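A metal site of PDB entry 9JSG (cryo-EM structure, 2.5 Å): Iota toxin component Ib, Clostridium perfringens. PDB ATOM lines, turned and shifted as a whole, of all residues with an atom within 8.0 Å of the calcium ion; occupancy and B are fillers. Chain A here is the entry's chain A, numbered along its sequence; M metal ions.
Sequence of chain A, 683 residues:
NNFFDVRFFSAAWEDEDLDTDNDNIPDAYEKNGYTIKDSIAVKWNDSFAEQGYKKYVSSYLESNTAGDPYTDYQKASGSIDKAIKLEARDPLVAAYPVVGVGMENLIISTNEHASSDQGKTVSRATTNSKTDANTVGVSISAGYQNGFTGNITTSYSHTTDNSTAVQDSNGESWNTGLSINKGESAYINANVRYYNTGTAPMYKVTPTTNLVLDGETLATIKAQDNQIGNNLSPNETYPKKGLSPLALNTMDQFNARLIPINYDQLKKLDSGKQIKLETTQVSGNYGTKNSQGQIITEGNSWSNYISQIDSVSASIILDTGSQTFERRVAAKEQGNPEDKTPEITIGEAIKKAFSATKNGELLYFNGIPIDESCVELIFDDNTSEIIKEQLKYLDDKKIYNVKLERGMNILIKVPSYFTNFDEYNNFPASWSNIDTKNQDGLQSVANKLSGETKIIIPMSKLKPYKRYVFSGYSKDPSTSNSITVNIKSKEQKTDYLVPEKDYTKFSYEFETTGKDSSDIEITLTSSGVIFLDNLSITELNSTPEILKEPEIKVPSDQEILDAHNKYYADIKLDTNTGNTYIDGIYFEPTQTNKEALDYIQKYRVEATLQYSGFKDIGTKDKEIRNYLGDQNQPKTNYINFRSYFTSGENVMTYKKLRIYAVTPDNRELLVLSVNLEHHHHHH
Residues that only touch the calcium ion: Gln 443 (3.9 Å) and Ser 444 (3.7 Å).
Six residues have an atom within 4 Å of the calcium ion: Asn 420, Asp 422, Gln 443, Ser 444, Val 445 and Asp 533.
The nearest printed residue that does not touch the calcium ion is Asn 534 (4.2 Å).
N of Asp 422 sits close to OD1 of Asn 420 (3.5 Å).
N of Val 445 sits close to OD1 of Asp 422.
OD1 of Asn 534 lies close to OE1 of Gln 443, at 3.1 Å.
The side-chain carboxylate (OD2) of Asp 533 lies close to the backbone NH (N) of Leu 442 (2.6 Å).
The calcium ion is bound by the backbone carbonyl oxygen of Asn 420 (2.6 Å), the backbone carbonyl oxygen of Val 445 (2.6 Å) and the side-chain carboxylate of Asp 533 (2.7 Å).
Slightly farther from the calcium ion lies OD2 of Asp 422 (2.9 Å).
Slightly farther from the calcium ion lies the side-chain carboxylate (OD1) of Asp 533 (3.0 Å).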
ATOM      1  N   PHE A 418       8.809  35.764  23.607  1.00  0.00           N
ATOM      2  CA  PHE A 418       9.263  34.394  23.418  1.00  0.00           C
ATOM      3  C   PHE A 418       8.609  33.490  24.461  1.00  0.00           C
ATOM      4  O   PHE A 418       8.381  33.892  25.603  1.00  0.00           O
ATOM      5  CB  PHE A 418      10.791  34.289  23.519  1.00  0.00           C
ATOM      6  CG  PHE A 418      11.320  32.891  23.317  1.00  0.00           C
ATOM      7  CD1 PHE A 418      11.392  32.351  22.050  1.00  0.00           C
ATOM      8  CD2 PHE A 418      11.737  32.134  24.397  1.00  0.00           C
ATOM      9  CE1 PHE A 418      11.884  31.071  21.861  1.00  0.00           C
ATOM     10  CE2 PHE A 418      12.229  30.854  24.208  1.00  0.00           C
ATOM     11  CZ  PHE A 418      12.295  30.320  22.939  1.00  0.00           C
ATOM     12  N   THR A 419       8.312  32.263  24.045  1.00  0.00           N
ATOM     13  CA  THR A 419       7.774  31.263  24.953  1.00  0.00           C
ATOM     14  C   THR A 419       8.300  29.891  24.552  1.00  0.00           C
ATOM     15  O   THR A 419       8.293  29.537  23.375  1.00  0.00           O
ATOM     16  CB  THR A 419       6.241  31.260  24.969  1.00  0.00           C
ATOM     17  OG1 THR A 419       5.768  30.124  25.705  1.00  0.00           O
ATOM     18  CG2 THR A 419       5.676  31.217  23.554  1.00  0.00           C
ATOM     19  N   ASN A 420       8.763  29.130  25.553  1.00  0.00           N
ATOM     20  CA  ASN A 420       9.210  27.758  25.385  1.00  0.00           C
ATOM     21  C   ASN A 420       8.387  26.783  26.218  1.00  0.00           C
ATOM     22  O   ASN A 420       8.690  25.588  26.241  1.00  0.00           O
ATOM     23  CB  ASN A 420      10.696  27.638  25.727  1.00  0.00           C
ATOM     24  CG  ASN A 420      11.007  28.114  27.126  1.00  0.00           C
ATOM     25  OD1 ASN A 420      10.163  28.705  27.807  1.00  0.00           O
ATOM     26  ND2 ASN A 420      12.228  27.853  27.580  1.00  0.00           N
ATOM     27  N   PHE A 421       7.367  27.274  26.924  1.00  0.00           N
ATOM     28  CA  PHE A 421       6.429  26.474  27.699  1.00  0.00           C
ATOM     29  C   PHE A 421       7.089  25.759  28.874  1.00  0.00           C
ATOM     30  O   PHE A 421       6.524  24.814  29.423  1.00  0.00           O
ATOM     31  CB  PHE A 421       5.706  25.446  26.812  1.00  0.00           C
ATOM     32  CG  PHE A 421       5.114  26.043  25.564  1.00  0.00           C
ATOM     33  CD1 PHE A 421       4.101  26.989  25.638  1.00  0.00           C
ATOM     34  CD2 PHE A 421       5.566  25.649  24.325  1.00  0.00           C
ATOM     35  CE1 PHE A 421       3.569  27.535  24.493  1.00  0.00           C
ATOM     36  CE2 PHE A 421       5.024  26.194  23.171  1.00  0.00           C
ATOM     37  CZ  PHE A 421       4.029  27.134  23.256  1.00  0.00           C
ATOM     38  N   ASP A 422       8.282  26.193  29.284  1.00  0.00           N
ATOM     39  CA  ASP A 422       8.976  25.597  30.417  1.00  0.00           C
ATOM     40  C   ASP A 422       9.092  26.554  31.592  1.00  0.00           C
ATOM     41  O   ASP A 422       8.600  26.255  32.691  1.00  0.00           O
ATOM     42  CB  ASP A 422      10.370  25.110  29.991  1.00  0.00           C
ATOM     43  CG  ASP A 422      10.333  24.289  28.721  1.00  0.00           C
ATOM     44  OD1 ASP A 422       9.285  23.673  28.433  1.00  0.00           O
ATOM     45  OD2 ASP A 422      11.355  24.259  27.997  1.00  0.00           O
ATOM     46  N   GLU A 423       9.739  27.708  31.407  1.00  0.00           N
ATOM     47  CA  GLU A 423       9.886  28.682  32.475  1.00  0.00           C
ATOM     48  C   GLU A 423       9.657  30.125  32.050  1.00  0.00           C
ATOM     49  O   GLU A 423       9.504  30.975  32.926  1.00  0.00           O
ATOM     50  CB  GLU A 423      11.282  28.571  33.120  1.00  0.00           C
ATOM     51  CG  GLU A 423      11.610  27.214  33.706  1.00  0.00           C
ATOM     52  CD  GLU A 423      12.442  27.312  34.973  1.00  0.00           C
ATOM     53  OE1 GLU A 423      12.291  28.318  35.703  1.00  0.00           O
ATOM     54  OE2 GLU A 423      13.243  26.389  35.239  1.00  0.00           O
ATOM     55  N   ASP A 440       7.824  15.798  24.433  1.00  0.00           N
ATOM     56  CA  ASP A 440       8.420  15.785  23.100  1.00  0.00           C
ATOM     57  C   ASP A 440       8.817  17.183  22.631  1.00  0.00           C
ATOM     58  O   ASP A 440       8.780  17.468  21.433  1.00  0.00           O
ATOM     59  CB  ASP A 440       7.451  15.152  22.096  1.00  0.00           C
ATOM     60  CG  ASP A 440       6.744  13.927  22.658  1.00  0.00           C
ATOM     61  OD1 ASP A 440       7.183  13.415  23.705  1.00  0.00           O
ATOM     62  OD2 ASP A 440       5.759  13.476  22.036  1.00  0.00           O
ATOM     63  N   GLY A 441       9.209  18.051  23.564  1.00  0.00           N
ATOM     64  CA  GLY A 441       9.529  19.415  23.212  1.00  0.00           C
ATOM     65  C   GLY A 441      10.918  19.592  22.656  1.00  0.00           C
ATOM     66  O   GLY A 441      11.748  18.676  22.651  1.00  0.00           O
ATOM     67  N   LEU A 442      11.162  20.803  22.149  1.00  0.00           N
ATOM     68  CA  LEU A 442      12.498  21.131  21.627  1.00  0.00           C
ATOM     69  C   LEU A 442      13.534  21.083  22.730  1.00  0.00           C
ATOM     70  O   LEU A 442      14.640  20.572  22.524  1.00  0.00           O
ATOM     71  CB  LEU A 442      12.469  22.506  20.953  1.00  0.00           C
ATOM     72  CG  LEU A 442      13.588  22.791  19.958  1.00  0.00           C
ATOM     73  CD1 LEU A 442      13.676  21.693  18.922  1.00  0.00           C
ATOM     74  CD2 LEU A 442      13.384  24.142  19.297  1.00  0.00           C
ATOM     75  N   GLN A 443      13.221  21.617  23.911  1.00  0.00           N
ATOM     76  CA  GLN A 443      14.126  21.572  25.051  1.00  0.00           C
ATOM     77  C   GLN A 443      13.578  20.727  26.187  1.00  0.00           C
ATOM     78  O   GLN A 443      14.218  19.741  26.584  1.00  0.00           O
ATOM     79  CB  GLN A 443      14.414  22.998  25.537  1.00  0.00           C
ATOM     80  CG  GLN A 443      15.394  23.768  24.665  1.00  0.00           C
ATOM     81  CD  GLN A 443      14.716  24.424  23.467  1.00  0.00           C
ATOM     82  OE1 GLN A 443      13.492  24.515  23.407  1.00  0.00           O
ATOM     83  NE2 GLN A 443      15.512  24.882  22.512  1.00  0.00           N
ATOM     84  N   SER A 444      12.414  21.069  26.742  1.00  0.00           N
ATOM     85  CA  SER A 444      11.804  20.286  27.810  1.00  0.00           C
ATOM     86  C   SER A 444      10.424  19.764  27.450  1.00  0.00           C
ATOM     87  O   SER A 444      10.198  18.548  27.498  1.00  0.00           O
ATOM     88  CB  SER A 444      11.752  21.120  29.100  1.00  0.00           C
ATOM     89  OG  SER A 444      11.400  20.318  30.209  1.00  0.00           O
ATOM     90  N   VAL A 445       9.495  20.648  27.083  1.00  0.00           N
ATOM     91  CA  VAL A 445       8.111  20.262  26.775  1.00  0.00           C
ATOM     92  C   VAL A 445       7.670  20.980  25.509  1.00  0.00           C
ATOM     93  O   VAL A 445       8.269  21.973  25.088  1.00  0.00           O
ATOM     94  CB  VAL A 445       7.132  20.574  27.933  1.00  0.00           C
ATOM     95  CG1 VAL A 445       7.791  20.383  29.297  1.00  0.00           C
ATOM     96  CG2 VAL A 445       6.563  21.974  27.803  1.00  0.00           C
ATOM     97  N   ALA A 446       6.614  20.450  24.896  1.00  0.00           N
ATOM     98  CA  ALA A 446       6.041  21.002  23.678  1.00  0.00           C
ATOM     99  C   ALA A 446       4.612  21.461  23.945  1.00  0.00           C
ATOM    100  O   ALA A 446       4.123  21.423  25.077  1.00  0.00           O
ATOM    101  CB  ALA A 446       6.104  19.982  22.540  1.00  0.00           C
ATOM    102  N   ASN A 447       3.936  21.881  22.876  1.00  0.00           N
ATOM    103  CA  ASN A 447       2.534  22.302  22.928  1.00  0.00           C
ATOM    104  C   ASN A 447       1.796  21.556  21.816  1.00  0.00           C
ATOM    105  O   ASN A 447       1.710  22.038  20.683  1.00  0.00           O
ATOM    106  CB  ASN A 447       2.412  23.815  22.776  1.00  0.00           C
ATOM    107  CG  ASN A 447       0.975  24.273  22.636  1.00  0.00           C
ATOM    108  OD1 ASN A 447       0.167  24.079  23.542  1.00  0.00           O
ATOM    109  ND2 ASN A 447       0.643  24.878  21.505  1.00  0.00           N
ATOM    110  N   TYR A 503      11.753  18.680  13.969  1.00  0.00           N
ATOM    111  CA  TYR A 503      11.417  20.078  14.214  1.00  0.00           C
ATOM    112  C   TYR A 503      11.969  20.968  13.107  1.00  0.00           C
ATOM    113  O   TYR A 503      13.131  20.847  12.714  1.00  0.00           O
ATOM    114  CB  TYR A 503      11.960  20.528  15.572  1.00  0.00           C
ATOM    115  CG  TYR A 503      10.969  20.415  16.706  1.00  0.00           C
ATOM    116  CD1 TYR A 503       9.864  21.254  16.768  1.00  0.00           C
ATOM    117  CD2 TYR A 503      11.115  19.463  17.702  1.00  0.00           C
ATOM    118  CE1 TYR A 503       8.941  21.154  17.794  1.00  0.00           C
ATOM    119  CE2 TYR A 503      10.210  19.356  18.739  1.00  0.00           C
ATOM    120  CZ  TYR A 503       9.123  20.207  18.781  1.00  0.00           C
ATOM    121  N   LEU A 532       4.212  22.139  18.751  1.00  0.00           N
ATOM    122  CA  LEU A 532       4.638  23.537  18.662  1.00  0.00           C
ATOM    123  C   LEU A 532       5.549  23.865  19.834  1.00  0.00           C
ATOM    124  O   LEU A 532       5.256  23.512  20.978  1.00  0.00           O
ATOM    125  CB  LEU A 532       3.428  24.477  18.643  1.00  0.00           C
ATOM    126  CG  LEU A 532       2.601  24.488  17.361  1.00  0.00           C
ATOM    127  CD1 LEU A 532       1.261  25.178  17.598  1.00  0.00           C
ATOM    128  CD2 LEU A 532       3.355  25.150  16.225  1.00  0.00           C
ATOM    129  N   ASP A 533       6.650  24.557  19.541  1.00  0.00           N
ATOM    130  CA  ASP A 533       7.586  24.936  20.593  1.00  0.00           C
ATOM    131  C   ASP A 533       8.362  26.168  20.148  1.00  0.00           C
ATOM    132  O   ASP A 533       8.550  26.416  18.953  1.00  0.00           O
ATOM    133  CB  ASP A 533       8.550  23.786  20.925  1.00  0.00           C
ATOM    134  CG  ASP A 533       8.971  23.788  22.383  1.00  0.00           C
ATOM    135  OD1 ASP A 533       8.467  24.635  23.141  1.00  0.00           O
ATOM    136  OD2 ASP A 533       9.812  22.945  22.759  1.00  0.00           O
ATOM    137  N   ASN A 534       8.816  26.927  21.150  1.00  0.00           N
ATOM    138  CA  ASN A 534       9.643  28.128  20.956  1.00  0.00           C
ATOM    139  C   ASN A 534       8.959  29.123  20.017  1.00  0.00           C
ATOM    140  O   ASN A 534       9.439  29.425  18.923  1.00  0.00           O
ATOM    141  CB  ASN A 534      11.038  27.752  20.441  1.00  0.00           C
ATOM    142  CG  ASN A 534      11.862  27.011  21.478  1.00  0.00           C
ATOM    143  OD1 ASN A 534      11.327  26.559  22.493  1.00  0.00           O
ATOM    144  ND2 ASN A 534      13.155  26.882  21.229  1.00  0.00           N
HETATM  145 CA    CA M   1      10.216  23.682  25.361  1.00  0.00          CA
